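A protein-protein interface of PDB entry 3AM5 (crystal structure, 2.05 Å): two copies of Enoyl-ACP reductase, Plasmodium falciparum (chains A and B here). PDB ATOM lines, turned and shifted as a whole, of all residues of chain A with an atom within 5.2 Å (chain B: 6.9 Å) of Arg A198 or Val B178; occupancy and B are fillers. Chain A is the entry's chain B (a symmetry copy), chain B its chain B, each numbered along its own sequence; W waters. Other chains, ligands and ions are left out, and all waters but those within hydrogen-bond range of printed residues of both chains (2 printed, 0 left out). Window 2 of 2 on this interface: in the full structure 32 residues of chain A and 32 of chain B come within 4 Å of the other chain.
O of Ser B175 sits at hydrogen-bond distance from OG of Ser A195, at 2.7 Å.
The backbone carbonyl oxygen (O) of Ser B175 is in hydrogen-bond range of the guanidinium group (NH2) of Arg A198 (2.9 Å).
The backbone carbonyl oxygen (O) of Gln B176 lies within hydrogen-bond range of the guanidinium group (NE) of Arg A198, 3.0 Å away.
The side-chain hydroxyl (OG) of Ser B175 lies within hydrogen-bond range of the side-chain amide oxygen (OE1) of Gln B176 (3.4 Å).
Among the printed residues, pairs that only touch across the chains: Ser A195 with Ala B191 (3.4 Å), Asp A196 with Leu B131 (3.5 Å), Arg A198 with Val B178 (3.5 Å), Val A199 with Leu B131 (3.7 Å), Tyr A202 with Pro B180 (3.8 Å), Tyr A202 with Val B178 (3.9 Å) and Val A199 with Val B178 (3.9 Å).
Arg A198 touches just these residues of chain B: Ser B175 (2.9 Å), Gln B176 (3.0 Å) and Val B178 (3.5 Å).
Printed residues of chain A within 4 Å of Leu B131: Asp A196 and Val A199.
Of the printed residues of chain A, Pro B180 touches Tyr A202.
Ala A201 touches none of the printed residues of chain B.
Glu A194 touches none of the printed residues of chain B.
The nearest residue of chain B that does not touch Arg A198 is Lys B177 (4.3 Å).
The nearest printed residue of chain A that does not touch Pro B180 is Val A199 (6.8 Å).
Hydrophobic or aromatic side chains of chain B within 4 Å of the printed part of chain A: Leu B131, Val B178, Pro B180 and Ala B191.
Hydrophobic or aromatic side chains of chain A within 4 Å of the printed part of chain B: Val A199 and Tyr A202.
No position is printed for both chains.
Of the 10 pairs that touch across the chains among the printed residues, none has its exchanged pair printed and touching as well.
Water W1 bridges the side-chain amide nitrogen of Gln B176 (2.9 Å) and the guanidinium group of Arg A198 (2.9 Å).
Water W2 lies within hydrogen-bond range of NE of Arg A198, OG of Ser A195, O of Ala B174 and O of Ser B175.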
ATOM      1  N   GLU A 194       8.629  19.345  27.230  1.00  0.00           N
ATOM      2  CA  GLU A 194       8.805  19.352  25.774  1.00  0.00           C
ATOM      3  C   GLU A 194      10.244  19.730  25.400  1.00  0.00           C
ATOM      4  O   GLU A 194      10.809  19.153  24.468  1.00  0.00           O
ATOM      5  CB  GLU A 194       7.794  20.310  25.127  1.00  0.00           C
ATOM      6  CG  GLU A 194       6.394  19.717  25.153  1.00  0.00           C
ATOM      7  CD  GLU A 194       5.332  20.700  24.749  1.00  0.00           C
ATOM      8  OE1 GLU A 194       5.618  21.567  23.898  1.00  0.00           O
ATOM      9  OE2 GLU A 194       4.201  20.598  25.274  1.00  0.00           O
ATOM     10  N   SER A 195      10.827  20.689  26.128  1.00  0.00           N
ATOM     11  CA  SER A 195      12.233  21.101  25.882  1.00  0.00           C
ATOM     12  C   SER A 195      13.206  19.984  26.328  1.00  0.00           C
ATOM     13  O   SER A 195      14.161  19.644  25.624  1.00  0.00           O
ATOM     14  CB  SER A 195      12.552  22.415  26.599  1.00  0.00           C
ATOM     15  OG  SER A 195      13.906  22.805  26.373  1.00  0.00           O
ATOM     16  N   ASP A 196      12.939  19.406  27.488  1.00  0.00           N
ATOM     17  CA  ASP A 196      13.740  18.298  28.011  1.00  0.00           C
ATOM     18  C   ASP A 196      13.698  17.079  27.089  1.00  0.00           C
ATOM     19  O   ASP A 196      14.673  16.295  27.029  1.00  0.00           O
ATOM     20  CB  ASP A 196      13.286  17.912  29.425  1.00  0.00           C
ATOM     21  CG  ASP A 196      13.532  19.026  30.455  1.00  0.00           C
ATOM     22  OD1 ASP A 196      14.261  20.014  30.127  1.00  0.00           O
ATOM     23  OD2 ASP A 196      12.999  18.890  31.604  1.00  0.00           O
ATOM     24  N   THR A 197      12.588  16.917  26.377  1.00  0.00           N
ATOM     25  CA  THR A 197      12.444  15.817  25.423  1.00  0.00           C
ATOM     26  C   THR A 197      13.488  15.942  24.303  1.00  0.00           C
ATOM     27  O   THR A 197      14.052  14.943  23.859  1.00  0.00           O
ATOM     28  CB  THR A 197      10.976  15.707  24.874  1.00  0.00           C
ATOM     29  OG1 THR A 197      10.101  15.359  25.973  1.00  0.00           O
ATOM     30  CG2 THR A 197      10.862  14.621  23.782  1.00  0.00           C
ATOM     31  N   ARG A 198      13.722  17.156  23.838  1.00  0.00           N
ATOM     32  CA  ARG A 198      14.753  17.400  22.829  1.00  0.00           C
ATOM     33  C   ARG A 198      16.134  17.120  23.408  1.00  0.00           C
ATOM     34  O   ARG A 198      16.945  16.401  22.801  1.00  0.00           O
ATOM     35  CB  ARG A 198      14.713  18.849  22.352  1.00  0.00           C
ATOM     36  CG  ARG A 198      13.541  19.133  21.471  1.00  0.00           C
ATOM     37  CD  ARG A 198      13.579  20.560  21.039  1.00  0.00           C
ATOM     38  NE  ARG A 198      13.180  21.544  22.056  1.00  0.00           N
ATOM     39  CZ  ARG A 198      11.931  21.933  22.257  1.00  0.00           C
ATOM     40  NH1 ARG A 198      10.953  21.383  21.544  1.00  0.00           N
ATOM     41  NH2 ARG A 198      11.660  22.874  23.158  1.00  0.00           N
ATOM     42  N   VAL A 199      16.413  17.687  24.583  1.00  0.00           N
ATOM     43  CA  VAL A 199      17.783  17.553  25.155  1.00  0.00           C
ATOM     44  C   VAL A 199      18.092  16.072  25.463  1.00  0.00           C
ATOM     45  O   VAL A 199      19.178  15.576  25.129  1.00  0.00           O
ATOM     46  CB  VAL A 199      17.986  18.439  26.400  1.00  0.00           C
ATOM     47  CG1 VAL A 199      19.430  18.279  26.983  1.00  0.00           C
ATOM     48  CG2 VAL A 199      17.701  19.891  26.031  1.00  0.00           C
ATOM     49  N   LEU A 200      17.138  15.376  26.069  1.00  0.00           N
ATOM     50  CA  LEU A 200      17.258  13.935  26.325  1.00  0.00           C
ATOM     51  C   LEU A 200      17.430  13.147  25.024  1.00  0.00           C
ATOM     52  O   LEU A 200      18.194  12.189  24.976  1.00  0.00           O
ATOM     53  CB  LEU A 200      16.046  13.418  27.103  1.00  0.00           C
ATOM     54  CG  LEU A 200      15.878  13.969  28.534  1.00  0.00           C
ATOM     55  CD1 LEU A 200      14.468  13.720  29.076  1.00  0.00           C
ATOM     56  CD2 LEU A 200      16.891  13.397  29.457  1.00  0.00           C
ATOM     57  N   ALA A 201      16.721  13.553  23.964  1.00  0.00           N
ATOM     58  CA  ALA A 201      16.821  12.876  22.685  1.00  0.00           C
ATOM     59  C   ALA A 201      18.262  12.899  22.166  1.00  0.00           C
ATOM     60  O   ALA A 201      18.752  11.913  21.594  1.00  0.00           O
ATOM     61  CB  ALA A 201      15.871  13.503  21.649  1.00  0.00           C
ATOM     62  N   TYR A 202      18.936  14.023  22.384  1.00  0.00           N
ATOM     63  CA  TYR A 202      20.327  14.178  21.976  1.00  0.00           C
ATOM     64  C   TYR A 202      21.214  13.214  22.755  1.00  0.00           C
ATOM     65  O   TYR A 202      21.899  12.376  22.169  1.00  0.00           O
ATOM     66  CB  TYR A 202      20.793  15.618  22.194  1.00  0.00           C
ATOM     67  CG  TYR A 202      22.297  15.779  22.211  1.00  0.00           C
ATOM     68  CD1 TYR A 202      23.034  15.716  21.036  1.00  0.00           C
ATOM     69  CD2 TYR A 202      22.978  15.994  23.401  1.00  0.00           C
ATOM     70  CE1 TYR A 202      24.409  15.863  21.046  1.00  0.00           C
ATOM     71  CE2 TYR A 202      24.352  16.142  23.422  1.00  0.00           C
ATOM     72  CZ  TYR A 202      25.062  16.076  22.242  1.00  0.00           C
ATOM     73  OH  TYR A 202      26.430  16.223  22.257  1.00  0.00           O
ATOM     74  N   GLY A 313      12.983  13.236  19.723  1.00  0.00           N
ATOM     75  CA  GLY A 313      13.016  14.610  20.224  1.00  0.00           C
ATOM     76  C   GLY A 313      11.756  15.404  19.911  1.00  0.00           C
ATOM     77  O   GLY A 313      11.718  16.594  20.163  1.00  0.00           O
ATOM     78  N   THR A 315       7.662  16.648  19.652  1.00  0.00           N
ATOM     79  CA  THR A 315       6.331  16.769  20.256  1.00  0.00           C
ATOM     80  C   THR A 315       5.298  16.441  19.160  1.00  0.00           C
ATOM     81  O   THR A 315       5.122  17.214  18.197  1.00  0.00           O
ATOM     82  CB  THR A 315       6.103  18.215  20.794  1.00  0.00           C
ATOM     83  OG1 THR A 315       7.004  18.447  21.875  1.00  0.00           O
ATOM     84  CG2 THR A 315       4.727  18.384  21.335  1.00  0.00           C
ATOM     85  N   LEU B 131      21.896  17.490  31.247  1.00  0.00           N
ATOM     86  CA  LEU B 131      20.544  17.399  31.789  1.00  0.00           C
ATOM     87  C   LEU B 131      20.317  16.014  32.369  1.00  0.00           C
ATOM     88  O   LEU B 131      19.792  15.885  33.464  1.00  0.00           O
ATOM     89  CB  LEU B 131      19.498  17.684  30.701  1.00  0.00           C
ATOM     90  CG  LEU B 131      18.018  17.790  31.141  1.00  0.00           C
ATOM     91  CD1 LEU B 131      17.792  18.943  32.127  1.00  0.00           C
ATOM     92  CD2 LEU B 131      17.033  17.927  29.912  1.00  0.00           C
ATOM     93  N   HIS B 173      18.143  30.506  23.440  1.00  0.00           N
ATOM     94  CA  HIS B 173      17.587  29.594  22.433  1.00  0.00           C
ATOM     95  C   HIS B 173      17.712  28.100  22.756  1.00  0.00           C
ATOM     96  O   HIS B 173      17.015  27.294  22.150  1.00  0.00           O
ATOM     97  CB  HIS B 173      18.267  29.908  21.077  1.00  0.00           C
ATOM     98  CG  HIS B 173      17.566  29.316  19.882  1.00  0.00           C
ATOM     99  ND1 HIS B 173      16.202  29.400  19.696  1.00  0.00           N
ATOM    100  CD2 HIS B 173      18.047  28.615  18.826  1.00  0.00           C
ATOM    101  CE1 HIS B 173      15.873  28.793  18.566  1.00  0.00           C
ATOM    102  NE2 HIS B 173      16.974  28.302  18.020  1.00  0.00           N
ATOM    103  N   ALA B 174      18.595  27.737  23.692  1.00  0.00           N
ATOM    104  CA  ALA B 174      18.688  26.357  24.180  1.00  0.00           C
ATOM    105  C   ALA B 174      17.355  25.795  24.700  1.00  0.00           C
ATOM    106  O   ALA B 174      17.230  24.577  24.852  1.00  0.00           O
ATOM    107  CB  ALA B 174      19.757  26.219  25.293  1.00  0.00           C
ATOM    108  N   SER B 175      16.392  26.675  25.003  1.00  0.00           N
ATOM    109  CA  SER B 175      15.030  26.263  25.403  1.00  0.00           C
ATOM    110  C   SER B 175      14.314  25.579  24.235  1.00  0.00           C
ATOM    111  O   SER B 175      13.497  24.692  24.432  1.00  0.00           O
ATOM    112  CB  SER B 175      14.202  27.499  25.810  1.00  0.00           C
ATOM    113  OG  SER B 175      14.196  28.406  24.708  1.00  0.00           O
ATOM    114  N   GLN B 176      14.642  25.980  23.014  1.00  0.00           N
ATOM    115  CA  GLN B 176      13.933  25.498  21.843  1.00  0.00           C
ATOM    116  C   GLN B 176      14.739  24.512  20.978  1.00  0.00           C
ATOM    117  O   GLN B 176      14.165  23.714  20.233  1.00  0.00           O
ATOM    118  CB  GLN B 176      13.521  26.690  20.950  1.00  0.00           C
ATOM    119  CG  GLN B 176      12.702  27.778  21.609  1.00  0.00           C
ATOM    120  CD  GLN B 176      11.486  27.211  22.356  1.00  0.00           C
ATOM    121  OE1 GLN B 176      11.160  27.637  23.466  1.00  0.00           O
ATOM    122  NE2 GLN B 176      10.840  26.231  21.758  1.00  0.00           N
ATOM    123  N   LYS B 177      16.070  24.619  21.017  1.00  0.00           N
ATOM    124  CA  LYS B 177      16.935  23.737  20.229  1.00  0.00           C
ATOM    125  C   LYS B 177      18.105  23.320  21.122  1.00  0.00           C
ATOM    126  O   LYS B 177      18.474  24.065  22.015  1.00  0.00           O
ATOM    127  CB  LYS B 177      17.478  24.455  18.987  1.00  0.00           C
ATOM    128  CG  LYS B 177      16.417  24.896  17.991  1.00  0.00           C
ATOM    129  CD  LYS B 177      15.729  23.702  17.347  1.00  0.00           C
ATOM    130  CE  LYS B 177      14.605  24.214  16.428  1.00  0.00           C
ATOM    131  NZ  LYS B 177      13.819  23.142  15.794  1.00  0.00           N
ATOM    132  N   VAL B 178      18.684  22.150  20.865  1.00  0.00           N
ATOM    133  CA  VAL B 178      19.628  21.561  21.791  1.00  0.00           C
ATOM    134  C   VAL B 178      20.996  22.235  21.697  1.00  0.00           C
ATOM    135  O   VAL B 178      21.569  22.374  20.592  1.00  0.00           O
ATOM    136  CB  VAL B 178      19.776  20.035  21.544  1.00  0.00           C
ATOM    137  CG1 VAL B 178      20.851  19.456  22.523  1.00  0.00           C
ATOM    138  CG2 VAL B 178      18.423  19.359  21.721  1.00  0.00           C
ATOM    139  N   VAL B 179      21.467  22.691  22.856  1.00  0.00           N
ATOM    140  CA  VAL B 179      22.780  23.292  22.998  1.00  0.00           C
ATOM    141  C   VAL B 179      23.520  22.457  24.030  1.00  0.00           C
ATOM    142  O   VAL B 179      23.262  22.553  25.243  1.00  0.00           O
ATOM    143  CB  VAL B 179      22.730  24.781  23.455  1.00  0.00           C
ATOM    144  CG1 VAL B 179      24.158  25.304  23.767  1.00  0.00           C
ATOM    145  CG2 VAL B 179      22.153  25.644  22.340  1.00  0.00           C
ATOM    146  N   PRO B 180      24.409  21.588  23.548  1.00  0.00           N
ATOM    147  CA  PRO B 180      25.202  20.783  24.477  1.00  0.00           C
ATOM    148  C   PRO B 180      26.047  21.739  25.311  1.00  0.00           C
ATOM    149  O   PRO B 180      26.587  22.727  24.789  1.00  0.00           O
ATOM    150  CB  PRO B 180      26.073  19.927  23.538  1.00  0.00           C
ATOM    151  CG  PRO B 180      25.268  19.846  22.278  1.00  0.00           C
ATOM    152  CD  PRO B 180      24.656  21.219  22.143  1.00  0.00           C
ATOM    153  N   TYR B 182      24.777  23.578  27.786  1.00  0.00           N
ATOM    154  CA  TYR B 182      23.842  24.432  28.545  1.00  0.00           C
ATOM    155  C   TYR B 182      23.088  23.549  29.524  1.00  0.00           C
ATOM    156  O   TYR B 182      21.939  23.164  29.287  1.00  0.00           O
ATOM    157  CB  TYR B 182      22.898  25.173  27.588  1.00  0.00           C
ATOM    158  CG  TYR B 182      22.221  26.404  28.177  1.00  0.00           C
ATOM    159  CD1 TYR B 182      22.955  27.557  28.482  1.00  0.00           C
ATOM    160  CD2 TYR B 182      20.854  26.425  28.413  1.00  0.00           C
ATOM    161  CE1 TYR B 182      22.317  28.717  29.001  1.00  0.00           C
ATOM    162  CE2 TYR B 182      20.208  27.586  28.914  1.00  0.00           C
ATOM    163  CZ  TYR B 182      20.944  28.707  29.193  1.00  0.00           C
ATOM    164  OH  TYR B 182      20.313  29.823  29.687  1.00  0.00           O
ATOM    165  N   ALA B 191      12.944  27.313  28.900  1.00  0.00           N
ATOM    166  CA  ALA B 191      11.700  26.860  28.274  1.00  0.00           C
ATOM    167  C   ALA B 191      10.461  27.249  29.131  1.00  0.00           C
ATOM    168  O   ALA B 191       9.459  27.730  28.600  1.00  0.00           O
ATOM    169  CB  ALA B 191      11.730  25.376  28.034  1.00  0.00           C
HETATM  170  O   HOH W   1       9.079  24.222  22.828  1.00  0.00           O
HETATM  171  O   HOH W   2      15.473  22.236  23.722  1.00  0.00           O
